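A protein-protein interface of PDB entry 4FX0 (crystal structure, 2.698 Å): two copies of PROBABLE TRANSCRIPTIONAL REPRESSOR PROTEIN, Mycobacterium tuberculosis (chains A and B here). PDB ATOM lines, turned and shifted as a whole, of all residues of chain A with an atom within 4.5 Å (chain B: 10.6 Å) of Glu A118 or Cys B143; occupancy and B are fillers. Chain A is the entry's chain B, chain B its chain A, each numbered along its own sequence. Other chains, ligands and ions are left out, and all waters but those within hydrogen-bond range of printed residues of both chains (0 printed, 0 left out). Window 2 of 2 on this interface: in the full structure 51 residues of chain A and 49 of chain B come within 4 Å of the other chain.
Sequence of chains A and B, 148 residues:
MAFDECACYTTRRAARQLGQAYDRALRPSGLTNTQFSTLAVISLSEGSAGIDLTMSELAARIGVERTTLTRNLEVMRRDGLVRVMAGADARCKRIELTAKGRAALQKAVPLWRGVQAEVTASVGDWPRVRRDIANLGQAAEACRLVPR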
ATOM      1  N   ALA A  21     -32.059  29.072  30.392  1.00  0.00           N
ATOM      2  CA  ALA A  21     -32.484  28.906  29.006  1.00  0.00           C
ATOM      3  C   ALA A  21     -33.298  27.628  28.825  1.00  0.00           C
ATOM      4  O   ALA A  21     -34.299  27.614  28.109  1.00  0.00           O
ATOM      5  CB  ALA A  21     -31.284  28.913  28.073  1.00  0.00           C
ATOM      6  N   ARG A  24     -36.707  28.216  30.280  1.00  0.00           N
ATOM      7  CA  ARG A  24     -37.473  29.028  29.343  1.00  0.00           C
ATOM      8  C   ARG A  24     -38.006  28.191  28.186  1.00  0.00           C
ATOM      9  O   ARG A  24     -39.180  28.285  27.831  1.00  0.00           O
ATOM     10  CB  ARG A  24     -36.617  30.175  28.804  1.00  0.00           C
ATOM     11  CG  ARG A  24     -37.327  31.023  27.765  1.00  0.00           C
ATOM     12  CD  ARG A  24     -36.381  32.001  27.091  1.00  0.00           C
ATOM     13  NE  ARG A  24     -37.060  32.763  26.048  1.00  0.00           N
ATOM     14  CZ  ARG A  24     -37.713  33.900  26.262  1.00  0.00           C
ATOM     15  NH1 ARG A  24     -37.775  34.411  27.484  1.00  0.00           N
ATOM     16  NH2 ARG A  24     -38.304  34.527  25.253  1.00  0.00           N
ATOM     17  N   GLY A 114     -34.462  21.350  20.887  1.00  0.00           N
ATOM     18  CA  GLY A 114     -34.235  22.596  20.179  1.00  0.00           C
ATOM     19  C   GLY A 114     -33.205  23.476  20.861  1.00  0.00           C
ATOM     20  O   GLY A 114     -32.316  24.022  20.210  1.00  0.00           O
ATOM     21  N   VAL A 115     -33.326  23.615  22.177  1.00  0.00           N
ATOM     22  CA  VAL A 115     -32.395  24.434  22.946  1.00  0.00           C
ATOM     23  C   VAL A 115     -31.011  23.788  22.994  1.00  0.00           C
ATOM     24  O   VAL A 115     -29.993  24.477  22.944  1.00  0.00           O
ATOM     25  CB  VAL A 115     -32.909  24.692  24.381  1.00  0.00           C
ATOM     26  CG1 VAL A 115     -33.056  23.384  25.143  1.00  0.00           C
ATOM     27  CG2 VAL A 115     -31.980  25.646  25.116  1.00  0.00           C
ATOM     28  N   GLN A 116     -30.984  22.461  23.085  1.00  0.00           N
ATOM     29  CA  GLN A 116     -29.735  21.709  23.074  1.00  0.00           C
ATOM     30  C   GLN A 116     -28.957  21.989  21.795  1.00  0.00           C
ATOM     31  O   GLN A 116     -27.753  22.244  21.829  1.00  0.00           O
ATOM     32  CB  GLN A 116     -30.023  20.210  23.183  1.00  0.00           C
ATOM     33  CG  GLN A 116     -28.793  19.318  23.091  1.00  0.00           C
ATOM     34  CD  GLN A 116     -28.033  19.226  24.399  1.00  0.00           C
ATOM     35  OE1 GLN A 116     -28.255  20.016  25.318  1.00  0.00           O
ATOM     36  NE2 GLN A 116     -27.135  18.252  24.493  1.00  0.00           N
ATOM     37  N   ALA A 117     -29.657  21.942  20.667  1.00  0.00           N
ATOM     38  CA  ALA A 117     -29.038  22.176  19.369  1.00  0.00           C
ATOM     39  C   ALA A 117     -28.537  23.611  19.242  1.00  0.00           C
ATOM     40  O   ALA A 117     -27.456  23.855  18.710  1.00  0.00           O
ATOM     41  CB  ALA A 117     -30.021  21.856  18.251  1.00  0.00           C
ATOM     42  N   GLU A 118     -29.330  24.553  19.739  1.00  0.00           N
ATOM     43  CA  GLU A 118     -29.010  25.972  19.626  1.00  0.00           C
ATOM     44  C   GLU A 118     -27.832  26.351  20.519  1.00  0.00           C
ATOM     45  O   GLU A 118     -27.043  27.234  20.181  1.00  0.00           O
ATOM     46  CB  GLU A 118     -30.239  26.816  19.976  1.00  0.00           C
ATOM     47  CG  GLU A 118     -30.141  28.276  19.563  1.00  0.00           C
ATOM     48  CD  GLU A 118     -31.457  29.013  19.733  1.00  0.00           C
ATOM     49  OE1 GLU A 118     -32.451  28.372  20.136  1.00  0.00           O
ATOM     50  OE2 GLU A 118     -31.499  30.232  19.462  1.00  0.00           O
ATOM     51  N   VAL A 119     -27.717  25.674  21.656  1.00  0.00           N
ATOM     52  CA  VAL A 119     -26.657  25.962  22.619  1.00  0.00           C
ATOM     53  C   VAL A 119     -25.332  25.288  22.260  1.00  0.00           C
ATOM     54  O   VAL A 119     -24.269  25.898  22.372  1.00  0.00           O
ATOM     55  CB  VAL A 119     -27.079  25.569  24.052  1.00  0.00           C
ATOM     56  CG1 VAL A 119     -25.870  25.192  24.890  1.00  0.00           C
ATOM     57  CG2 VAL A 119     -27.860  26.703  24.702  1.00  0.00           C
ATOM     58  N   THR A 120     -25.401  24.033  21.822  1.00  0.00           N
ATOM     59  CA  THR A 120     -24.198  23.276  21.489  1.00  0.00           C
ATOM     60  C   THR A 120     -23.665  23.623  20.100  1.00  0.00           C
ATOM     61  O   THR A 120     -22.711  23.009  19.620  1.00  0.00           O
ATOM     62  CB  THR A 120     -24.440  21.758  21.576  1.00  0.00           C
ATOM     63  OG1 THR A 120     -25.458  21.379  20.642  1.00  0.00           O
ATOM     64  CG2 THR A 120     -24.875  21.368  22.981  1.00  0.00           C
ATOM     65  N   ALA A 121     -24.288  24.604  19.457  1.00  0.00           N
ATOM     66  CA  ALA A 121     -23.815  25.088  18.167  1.00  0.00           C
ATOM     67  C   ALA A 121     -22.757  26.163  18.387  1.00  0.00           C
ATOM     68  O   ALA A 121     -22.137  26.652  17.442  1.00  0.00           O
ATOM     69  CB  ALA A 121     -24.972  25.633  17.348  1.00  0.00           C
ATOM     70  N   ALA B   7     -26.511  19.134  27.597  1.00  0.00           N
ATOM     71  CA  ALA B   7     -25.539  20.150  27.973  1.00  0.00           C
ATOM     72  C   ALA B   7     -25.834  20.707  29.359  1.00  0.00           C
ATOM     73  O   ALA B   7     -24.923  21.095  30.091  1.00  0.00           O
ATOM     74  CB  ALA B   7     -25.523  21.268  26.946  1.00  0.00           C
ATOM     75  N   ASP B 132     -14.929  27.335  25.724  1.00  0.00           N
ATOM     76  CA  ASP B 132     -16.059  26.517  25.291  1.00  0.00           C
ATOM     77  C   ASP B 132     -17.191  26.529  26.314  1.00  0.00           C
ATOM     78  O   ASP B 132     -18.357  26.691  25.956  1.00  0.00           O
ATOM     79  CB  ASP B 132     -15.622  25.078  25.002  1.00  0.00           C
ATOM     80  CG  ASP B 132     -14.926  24.937  23.659  1.00  0.00           C
ATOM     81  OD1 ASP B 132     -15.124  25.811  22.788  1.00  0.00           O
ATOM     82  OD2 ASP B 132     -14.188  23.947  23.473  1.00  0.00           O
ATOM     83  N   ASN B 135     -18.696  29.948  26.361  1.00  0.00           N
ATOM     84  CA  ASN B 135     -19.475  30.043  25.134  1.00  0.00           C
ATOM     85  C   ASN B 135     -20.792  29.298  25.276  1.00  0.00           C
ATOM     86  O   ASN B 135     -21.825  29.731  24.767  1.00  0.00           O
ATOM     87  CB  ASN B 135     -18.685  29.478  23.955  1.00  0.00           C
ATOM     88  CG  ASN B 135     -17.570  30.397  23.507  1.00  0.00           C
ATOM     89  OD1 ASN B 135     -17.330  31.443  24.111  1.00  0.00           O
ATOM     90  ND2 ASN B 135     -16.877  30.009  22.443  1.00  0.00           N
ATOM     91  N   LEU B 136     -20.742  28.172  25.977  1.00  0.00           N
ATOM     92  CA  LEU B 136     -21.924  27.362  26.218  1.00  0.00           C
ATOM     93  C   LEU B 136     -22.963  28.160  26.998  1.00  0.00           C
ATOM     94  O   LEU B 136     -24.087  28.355  26.534  1.00  0.00           O
ATOM     95  CB  LEU B 136     -21.541  26.093  26.979  1.00  0.00           C
ATOM     96  CG  LEU B 136     -22.058  24.770  26.412  1.00  0.00           C
ATOM     97  CD1 LEU B 136     -21.877  24.719  24.902  1.00  0.00           C
ATOM     98  CD2 LEU B 136     -21.359  23.598  27.087  1.00  0.00           C
ATOM     99  N   GLY B 137     -22.577  28.627  28.183  1.00  0.00           N
ATOM    100  CA  GLY B 137     -23.452  29.451  28.996  1.00  0.00           C
ATOM    101  C   GLY B 137     -23.830  30.721  28.263  1.00  0.00           C
ATOM    102  O   GLY B 137     -24.952  31.212  28.374  1.00  0.00           O
ATOM    103  N   GLN B 138     -22.878  31.251  27.504  1.00  0.00           N
ATOM    104  CA  GLN B 138     -23.106  32.444  26.704  1.00  0.00           C
ATOM    105  C   GLN B 138     -24.161  32.185  25.636  1.00  0.00           C
ATOM    106  O   GLN B 138     -25.038  33.018  25.400  1.00  0.00           O
ATOM    107  CB  GLN B 138     -21.799  32.884  26.053  1.00  0.00           C
ATOM    108  CG  GLN B 138     -21.943  34.009  25.060  1.00  0.00           C
ATOM    109  CD  GLN B 138     -20.615  34.391  24.449  1.00  0.00           C
ATOM    110  OE1 GLN B 138     -19.681  34.771  25.154  1.00  0.00           O
ATOM    111  NE2 GLN B 138     -20.518  34.275  23.130  1.00  0.00           N
ATOM    112  N   ALA B 139     -24.068  31.024  24.994  1.00  0.00           N
ATOM    113  CA  ALA B 139     -25.047  30.619  23.996  1.00  0.00           C
ATOM    114  C   ALA B 139     -26.427  30.593  24.628  1.00  0.00           C
ATOM    115  O   ALA B 139     -27.398  31.085  24.053  1.00  0.00           O
ATOM    116  CB  ALA B 139     -24.698  29.250  23.436  1.00  0.00           C
ATOM    117  N   ALA B 140     -26.502  30.020  25.825  1.00  0.00           N
ATOM    118  CA  ALA B 140     -27.756  29.934  26.559  1.00  0.00           C
ATOM    119  C   ALA B 140     -28.319  31.324  26.824  1.00  0.00           C
ATOM    120  O   ALA B 140     -29.474  31.608  26.506  1.00  0.00           O
ATOM    121  CB  ALA B 140     -27.547  29.190  27.865  1.00  0.00           C
ATOM    122  N   GLU B 141     -27.490  32.185  27.408  1.00  0.00           N
ATOM    123  CA  GLU B 141     -27.885  33.551  27.727  1.00  0.00           C
ATOM    124  C   GLU B 141     -28.562  34.228  26.538  1.00  0.00           C
ATOM    125  O   GLU B 141     -29.629  34.824  26.679  1.00  0.00           O
ATOM    126  CB  GLU B 141     -26.668  34.366  28.165  1.00  0.00           C
ATOM    127  CG  GLU B 141     -26.999  35.743  28.715  1.00  0.00           C
ATOM    128  CD  GLU B 141     -27.365  35.712  30.186  1.00  0.00           C
ATOM    129  OE1 GLU B 141     -26.861  36.572  30.938  1.00  0.00           O
ATOM    130  OE2 GLU B 141     -28.153  34.831  30.593  1.00  0.00           O
ATOM    131  N   ALA B 142     -27.935  34.133  25.369  1.00  0.00           N
ATOM    132  CA  ALA B 142     -28.487  34.731  24.159  1.00  0.00           C
ATOM    133  C   ALA B 142     -29.931  34.291  23.932  1.00  0.00           C
ATOM    134  O   ALA B 142     -30.754  35.058  23.437  1.00  0.00           O
ATOM    135  CB  ALA B 142     -27.628  34.383  22.954  1.00  0.00           C
ATOM    136  N   CYS B 143     -30.233  33.050  24.301  1.00  0.00           N
ATOM    137  CA  CYS B 143     -31.585  32.521  24.171  1.00  0.00           C
ATOM    138  C   CYS B 143     -32.469  33.002  25.317  1.00  0.00           C
ATOM    139  O   CYS B 143     -33.307  33.886  25.140  1.00  0.00           O
ATOM    140  CB  CYS B 143     -31.563  30.992  24.135  1.00  0.00           C
ATOM    141  SG  CYS B 143     -30.586  30.287  22.788  1.00  0.00           S
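The side-chain sulfur (SG) of Cys B143 sits at hydrogen-bond distance from the backbone carbonyl oxygen (O) of Ala B139.
O of Gln A116 is in hydrogen-bond range of OG1 of Thr A120 (2.7 Å).
No position is printed for both chains.
Of the 6 pairs that touch across the chains among the printed residues, none has its exchanged pair printed and touching as well.
Of chain B, only Cys B143 (3.4 Å) comes within 4 Å of Glu A118.
Of chain A, only Glu A118 comes within 4 Å of Cys B143.
No residue of chain B comes within 4 Å of Gly A114.
Ala A117 touches none of the printed residues of chain B.
No residue of chain B comes within 4 Å of Ala A121.
Of the printed residues of chain A, Ala B139 touches Val A119.
Printed residues of chain B within 4 Å of Gln A116: Ala B7.
Printed residues of chain A within 4 Å of Ala B7: Gln A116 (3.0 Å).
Gln B138 touches none of the printed residues of chain A.
The nearest residue of chain B that does not touch Glu A118 is Ala B139 (4.5 Å).
The nearest residue of chain A that does not touch Cys B143 is Arg A24 (4.02 Å).
The nearest printed residue of chain A that does not touch Ala B140 is Val A115 (6.2 Å).
Hydrophobic or aromatic side chains of chain B that line the printed part of chain A: Ala B7, Leu B136, Ala B139 and Ala B140.
Of the 10 printed residues of chain A, 4 touch a printed residue of chain B.
Hydrophobic or aromatic side chains of chain A within 4 Å of the printed part of chain B: Ala A21 and Val A119.
OE1 of Gln A116 is in hydrogen-bond range of N of Ala B7.
OE2 of Glu A118 lies close to SG of Cys B143, 3.4 Å away.
Ala B140 touches Ala A21.
Val A119 touches Leu B136 (O to CD1, 3.7 Å).
Ala B139 touches Val A119.
CG2 of Val A119 touches CA of Ala B140, at 3.7 Å.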
